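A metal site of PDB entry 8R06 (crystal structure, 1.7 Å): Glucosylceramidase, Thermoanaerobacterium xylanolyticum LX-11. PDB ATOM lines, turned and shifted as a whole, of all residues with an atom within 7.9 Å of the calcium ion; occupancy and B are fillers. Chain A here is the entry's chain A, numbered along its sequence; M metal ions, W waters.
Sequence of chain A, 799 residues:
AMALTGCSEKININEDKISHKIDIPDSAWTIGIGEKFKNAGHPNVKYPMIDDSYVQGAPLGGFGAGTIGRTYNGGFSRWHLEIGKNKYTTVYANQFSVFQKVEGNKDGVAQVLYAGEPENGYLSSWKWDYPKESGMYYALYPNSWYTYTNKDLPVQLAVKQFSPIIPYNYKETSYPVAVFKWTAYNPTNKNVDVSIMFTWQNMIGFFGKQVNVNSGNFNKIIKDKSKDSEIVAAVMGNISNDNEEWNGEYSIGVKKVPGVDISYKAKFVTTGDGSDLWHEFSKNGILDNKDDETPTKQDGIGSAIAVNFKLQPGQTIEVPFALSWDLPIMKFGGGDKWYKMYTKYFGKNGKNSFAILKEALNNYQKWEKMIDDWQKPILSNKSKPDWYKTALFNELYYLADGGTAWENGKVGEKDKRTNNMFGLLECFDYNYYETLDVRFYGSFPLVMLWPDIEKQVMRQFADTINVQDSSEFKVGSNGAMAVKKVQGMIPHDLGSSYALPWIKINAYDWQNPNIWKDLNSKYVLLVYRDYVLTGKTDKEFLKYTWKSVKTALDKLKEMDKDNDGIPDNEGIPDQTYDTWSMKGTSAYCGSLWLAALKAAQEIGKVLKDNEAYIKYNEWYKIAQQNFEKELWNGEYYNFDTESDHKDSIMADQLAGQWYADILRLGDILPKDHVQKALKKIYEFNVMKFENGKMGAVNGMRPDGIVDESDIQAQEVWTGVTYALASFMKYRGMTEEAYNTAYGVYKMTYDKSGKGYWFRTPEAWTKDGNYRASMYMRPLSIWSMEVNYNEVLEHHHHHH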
ATOM      1  N   LYS A 557       3.455  11.677  -3.917  1.00  0.00           N
ATOM      2  CA  LYS A 557       4.103  11.164  -5.114  1.00  0.00           C
ATOM      3  C   LYS A 557       3.054  10.741  -6.161  1.00  0.00           C
ATOM      4  O   LYS A 557       3.279  10.929  -7.343  1.00  0.00           O
ATOM      5  CB  LYS A 557       4.997   9.975  -4.787  1.00  0.00           C
ATOM      6  CG  LYS A 557       5.821   9.415  -5.975  1.00  0.00           C
ATOM      7  CD  LYS A 557       6.611  10.519  -6.659  1.00  0.00           C
ATOM      8  CE  LYS A 557       7.907  10.083  -7.250  1.00  0.00           C
ATOM      9  NZ  LYS A 557       7.669   9.127  -8.319  1.00  0.00           N
ATOM     10  N   MET A 559       0.533  12.122  -6.967  1.00  0.00           N
ATOM     11  CA  MET A 559      -0.053  13.252  -7.674  1.00  0.00           C
ATOM     12  C   MET A 559       0.859  13.759  -8.786  1.00  0.00           C
ATOM     13  O   MET A 559       0.560  14.770  -9.437  1.00  0.00           O
ATOM     14  CB  MET A 559      -0.414  14.368  -6.689  1.00  0.00           C
ATOM     15  CG  MET A 559      -1.599  14.000  -5.855  1.00  0.00           C
ATOM     16  SD  MET A 559      -1.785  15.229  -4.537  1.00  0.00           S
ATOM     17  CE  MET A 559      -3.079  14.372  -3.606  1.00  0.00           C
ATOM     18  N   ASP A 560       1.963  13.042  -9.045  1.00  0.00           N
ATOM     19  CA  ASP A 560       2.845  13.374 -10.151  1.00  0.00           C
ATOM     20  C   ASP A 560       2.299  12.743 -11.419  1.00  0.00           C
ATOM     21  O   ASP A 560       2.680  11.625 -11.741  1.00  0.00           O
ATOM     22  CB  ASP A 560       4.228  12.807  -9.901  1.00  0.00           C
ATOM     23  CG  ASP A 560       5.212  12.951 -11.052  1.00  0.00           C
ATOM     24  OD1 ASP A 560       4.992  13.814 -11.906  1.00  0.00           O
ATOM     25  OD2 ASP A 560       6.168  12.197 -11.057  1.00  0.00           O
ATOM     26  N   LYS A 561       1.452  13.487 -12.129  1.00  0.00           N
ATOM     27  CA  LYS A 561       0.726  12.991 -13.287  1.00  0.00           C
ATOM     28  C   LYS A 561       1.667  12.837 -14.490  1.00  0.00           C
ATOM     29  O   LYS A 561       1.548  11.867 -15.238  1.00  0.00           O
ATOM     30  CB  LYS A 561      -0.420  13.964 -13.618  1.00  0.00           C
ATOM     31  CG  LYS A 561      -1.792  13.716 -12.953  1.00  0.00           C
ATOM     32  CD  LYS A 561      -1.860  12.798 -11.732  1.00  0.00           C
ATOM     33  CE  LYS A 561      -1.974  11.333 -12.081  1.00  0.00           C
ATOM     34  NZ  LYS A 561      -1.472  10.497 -10.985  1.00  0.00           N
ATOM     35  N   ASP A 562       2.590  13.786 -14.671  1.00  0.00           N
ATOM     36  CA  ASP A 562       3.387  13.882 -15.893  1.00  0.00           C
ATOM     37  C   ASP A 562       4.717  13.139 -15.752  1.00  0.00           C
ATOM     38  O   ASP A 562       5.572  13.276 -16.612  1.00  0.00           O
ATOM     39  CB  ASP A 562       3.607  15.339 -16.291  1.00  0.00           C
ATOM     40  CG  ASP A 562       4.407  16.179 -15.301  1.00  0.00           C
ATOM     41  OD1 ASP A 562       5.004  15.589 -14.391  1.00  0.00           O
ATOM     42  OD2 ASP A 562       4.411  17.427 -15.423  1.00  0.00           O
ATOM     43  N   ASN A 563       4.914  12.441 -14.631  1.00  0.00           N
ATOM     44  CA  ASN A 563       6.072  11.612 -14.345  1.00  0.00           C
ATOM     45  C   ASN A 563       7.415  12.354 -14.437  1.00  0.00           C
ATOM     46  O   ASN A 563       8.421  11.776 -14.859  1.00  0.00           O
ATOM     47  CB  ASN A 563       6.053  10.335 -15.189  1.00  0.00           C
ATOM     48  CG  ASN A 563       6.882   9.238 -14.571  1.00  0.00           C
ATOM     49  OD1 ASN A 563       7.138   9.234 -13.358  1.00  0.00           O
ATOM     50  ND2 ASN A 563       7.316   8.282 -15.372  1.00  0.00           N
ATOM     51  N   ASP A 564       7.492  13.605 -13.958  1.00  0.00           N
ATOM     52  CA  ASP A 564       8.781  14.284 -13.829  1.00  0.00           C
ATOM     53  C   ASP A 564       9.309  14.152 -12.401  1.00  0.00           C
ATOM     54  O   ASP A 564      10.316  14.781 -12.063  1.00  0.00           O
ATOM     55  CB  ASP A 564       8.693  15.748 -14.213  1.00  0.00           C
ATOM     56  CG  ASP A 564       7.852  16.597 -13.255  1.00  0.00           C
ATOM     57  OD1 ASP A 564       7.255  15.998 -12.346  1.00  0.00           O
ATOM     58  OD2 ASP A 564       7.794  17.836 -13.435  1.00  0.00           O
ATOM     59  N   GLY A 565       8.635  13.348 -11.557  1.00  0.00           N
ATOM     60  CA  GLY A 565       9.113  13.108 -10.191  1.00  0.00           C
ATOM     61  C   GLY A 565       8.564  14.114  -9.153  1.00  0.00           C
ATOM     62  O   GLY A 565       8.889  13.999  -7.968  1.00  0.00           O
ATOM     63  N   ILE A 566       7.709  15.057  -9.568  1.00  0.00           N
ATOM     64  CA  ILE A 566       7.215  16.132  -8.716  1.00  0.00           C
ATOM     65  C   ILE A 566       5.693  16.154  -8.720  1.00  0.00           C
ATOM     66  O   ILE A 566       5.069  16.052  -9.757  1.00  0.00           O
ATOM     67  CB  ILE A 566       7.781  17.488  -9.197  1.00  0.00           C
ATOM     68  CG1 ILE A 566       9.314  17.433  -9.330  1.00  0.00           C
ATOM     69  CG2 ILE A 566       7.353  18.647  -8.296  1.00  0.00           C
ATOM     70  CD1 ILE A 566       9.880  18.584 -10.106  1.00  0.00           C
ATOM     71  N   PRO A 567       4.974  16.336  -7.600  1.00  0.00           N
ATOM     72  CA  PRO A 567       3.524  16.469  -7.682  1.00  0.00           C
ATOM     73  C   PRO A 567       3.108  17.632  -8.585  1.00  0.00           C
ATOM     74  O   PRO A 567       3.755  18.664  -8.615  1.00  0.00           O
ATOM     75  CB  PRO A 567       3.076  16.676  -6.216  1.00  0.00           C
ATOM     76  CG  PRO A 567       4.339  17.041  -5.480  1.00  0.00           C
ATOM     77  CD  PRO A 567       5.511  16.447  -6.248  1.00  0.00           C
ATOM     78  N   ASP A 568       2.014  17.470  -9.347  1.00  0.00           N
ATOM     79  CA  ASP A 568       1.597  18.497 -10.297  1.00  0.00           C
ATOM     80  C   ASP A 568       0.482  19.353  -9.717  1.00  0.00           C
ATOM     81  O   ASP A 568      -0.545  18.816  -9.323  1.00  0.00           O
ATOM     82  CB  ASP A 568       0.962  17.901 -11.544  1.00  0.00           C
ATOM     83  CG  ASP A 568       1.935  17.125 -12.402  1.00  0.00           C
ATOM     84  OD1 ASP A 568       2.586  16.219 -11.855  1.00  0.00           O
ATOM     85  OD2 ASP A 568       2.089  17.506 -13.581  1.00  0.00           O
ATOM     86  N   ASN A 569       0.653  20.674  -9.764  1.00  0.00           N
ATOM     87  CA  ASN A 569      -0.468  21.541  -9.413  1.00  0.00           C
ATOM     88  C   ASN A 569      -1.474  21.478 -10.554  1.00  0.00           C
ATOM     89  O   ASN A 569      -1.064  21.378 -11.723  1.00  0.00           O
ATOM     90  CB  ASN A 569      -0.068  22.988  -9.131  1.00  0.00           C
ATOM     91  CG  ASN A 569       0.757  23.138  -7.872  1.00  0.00           C
ATOM     92  OD1 ASN A 569       0.210  23.244  -6.762  1.00  0.00           O
ATOM     93  ND2 ASN A 569       2.073  23.132  -8.021  1.00  0.00           N
ATOM     94  N   GLY A 584       1.086  22.691 -13.226  1.00  0.00           N
ATOM     95  CA  GLY A 584       2.273  21.947 -13.614  1.00  0.00           C
ATOM     96  C   GLY A 584       3.200  21.793 -12.407  1.00  0.00           C
ATOM     97  O   GLY A 584       2.737  21.473 -11.306  1.00  0.00           O
ATOM     98  N   THR A 585       4.490  22.026 -12.622  1.00  0.00           N
ATOM     99  CA  THR A 585       5.405  22.138 -11.509  1.00  0.00           C
ATOM    100  C   THR A 585       5.483  23.598 -11.059  1.00  0.00           C
ATOM    101  O   THR A 585       5.738  24.493 -11.864  1.00  0.00           O
ATOM    102  CB  THR A 585       6.803  21.646 -11.911  1.00  0.00           C
ATOM    103  OG1 THR A 585       6.649  20.258 -12.185  1.00  0.00           O
ATOM    104  CG2 THR A 585       7.807  21.888 -10.798  1.00  0.00           C
ATOM    105  N   TRP A 593       8.588  20.064  -1.795  1.00  0.00           N
ATOM    106  CA  TRP A 593       8.715  18.644  -2.049  1.00  0.00           C
ATOM    107  C   TRP A 593      10.184  18.215  -2.018  1.00  0.00           C
ATOM    108  O   TRP A 593      10.511  17.213  -1.397  1.00  0.00           O
ATOM    109  CB  TRP A 593       8.049  18.372  -3.397  1.00  0.00           C
ATOM    110  CG  TRP A 593       8.259  17.014  -3.973  1.00  0.00           C
ATOM    111  CD1 TRP A 593       8.943  16.725  -5.118  1.00  0.00           C
ATOM    112  CD2 TRP A 593       7.704  15.774  -3.490  1.00  0.00           C
ATOM    113  NE1 TRP A 593       8.872  15.384  -5.350  1.00  0.00           N
ATOM    114  CE2 TRP A 593       8.114  14.769  -4.399  1.00  0.00           C
ATOM    115  CE3 TRP A 593       6.901  15.418  -2.411  1.00  0.00           C
ATOM    116  CZ2 TRP A 593       7.777  13.435  -4.229  1.00  0.00           C
ATOM    117  CZ3 TRP A 593       6.550  14.102  -2.241  1.00  0.00           C
ATOM    118  CH2 TRP A 593       6.978  13.122  -3.148  1.00  0.00           C
ATOM    119  N   ASN A 626      14.852  17.777 -12.621  1.00  0.00           N
ATOM    120  CA  ASN A 626      13.716  18.265 -13.380  1.00  0.00           C
ATOM    121  C   ASN A 626      13.224  19.632 -12.898  1.00  0.00           C
ATOM    122  O   ASN A 626      12.784  20.422 -13.730  1.00  0.00           O
ATOM    123  CB  ASN A 626      12.595  17.236 -13.388  1.00  0.00           C
ATOM    124  CG  ASN A 626      12.966  16.099 -14.306  1.00  0.00           C
ATOM    125  OD1 ASN A 626      13.805  16.270 -15.193  1.00  0.00           O
ATOM    126  ND2 ASN A 626      12.373  14.936 -14.107  1.00  0.00           N
ATOM    127  N   GLU A 630      13.043  22.707 -15.437  1.00  0.00           N
ATOM    128  CA  GLU A 630      11.728  23.246 -15.721  1.00  0.00           C
ATOM    129  C   GLU A 630      11.645  24.724 -15.351  1.00  0.00           C
ATOM    130  O   GLU A 630      10.896  25.453 -15.968  1.00  0.00           O
ATOM    131  CB  GLU A 630      10.686  22.412 -14.986  1.00  0.00           C
ATOM    132  CG  GLU A 630      10.420  21.082 -15.669  1.00  0.00           C
ATOM    133  CD  GLU A 630       9.596  20.168 -14.774  1.00  0.00           C
ATOM    134  OE1 GLU A 630       9.103  20.688 -13.744  1.00  0.00           O
ATOM    135  OE2 GLU A 630       9.487  18.956 -15.038  1.00  0.00           O
ATOM    136  N   THR A 641       5.194  26.061 -14.406  1.00  0.00           N
ATOM    137  CA  THR A 641       5.518  25.635 -15.767  1.00  0.00           C
ATOM    138  C   THR A 641       4.366  25.866 -16.754  1.00  0.00           C
ATOM    139  O   THR A 641       4.655  25.855 -17.938  1.00  0.00           O
ATOM    140  CB  THR A 641       5.938  24.170 -15.831  1.00  0.00           C
ATOM    141  OG1 THR A 641       4.922  23.326 -15.300  1.00  0.00           O
ATOM    142  CG2 THR A 641       7.275  23.954 -15.153  1.00  0.00           C
ATOM    143  N   GLU A 642       3.113  26.058 -16.318  1.00  0.00           N
ATOM    144  CA  GLU A 642       1.991  26.026 -17.260  1.00  0.00           C
ATOM    145  C   GLU A 642       0.961  27.159 -17.109  1.00  0.00           C
ATOM    146  O   GLU A 642       0.064  27.243 -17.937  1.00  0.00           O
ATOM    147  CB  GLU A 642       1.255  24.689 -17.168  1.00  0.00           C
ATOM    148  CG  GLU A 642       2.085  23.491 -17.649  1.00  0.00           C
ATOM    149  CD  GLU A 642       1.401  22.162 -17.372  1.00  0.00           C
ATOM    150  OE1 GLU A 642       0.172  22.120 -17.585  1.00  0.00           O
ATOM    151  OE2 GLU A 642       2.042  21.169 -16.941  1.00  0.00           O
HETATM  152 CA    CA M   1       4.929  16.200 -12.072  1.00  0.00          CA
HETATM  153  O   HOH W   1       5.119  18.552 -11.637  1.00  0.00           O
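The side-chain carboxylate (OE2) of Glu 630 sits close to the side-chain carboxylate (OD2) of Asp 564 (2.6 Å). The backbone carbonyl oxygen (O) of Met 559 lies within hydrogen-bond range of the backbone NH (N) of Asp 568. OD1 of Asp 560 sits close to N of Asn 563, at 3.1 Å. The backbone NH (N) of Lys 561 sits close to the side-chain carboxylate (OD1) of Asp 568, at 3.0 Å. O of Asp 564 is in hydrogen-bond range of ND2 of Asn 626 (2.9 Å). The backbone NH (N) of Gly 565 lies within hydrogen-bond range of the side-chain carboxylate (OD2) of Asp 560 (2.8 Å). The side-chain carboxylate (OD2) of Asp 564 sits at hydrogen-bond distance from the side-chain hydroxyl (OG1) of Thr 585.
Water W1 lies within hydrogen-bond range of the side-chain carboxylate (OD2) of Asp 564 (3.3 Å) and the backbone carbonyl oxygen (O) of Pro 567 (3.3 Å).
The calcium ion is bound by the backbone carbonyl oxygen (O) of Ile 566 (2.3 Å), the side-chain carboxylate (OD1) of Asp 564 (2.4 Å), the side-chain carboxylate (OD1) of Asp 568 (2.4 Å), the side-chain carboxylate (OD1) of Asp 560 (2.4 Å), the side-chain carboxylate (OD1) of Asp 562 (2.4 Å) and water W1 (2.4 Å). The calcium ion has six donor atoms within binding distance.
Of the 19 residues printed, 5 come within 4 Å of the calcium ion.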
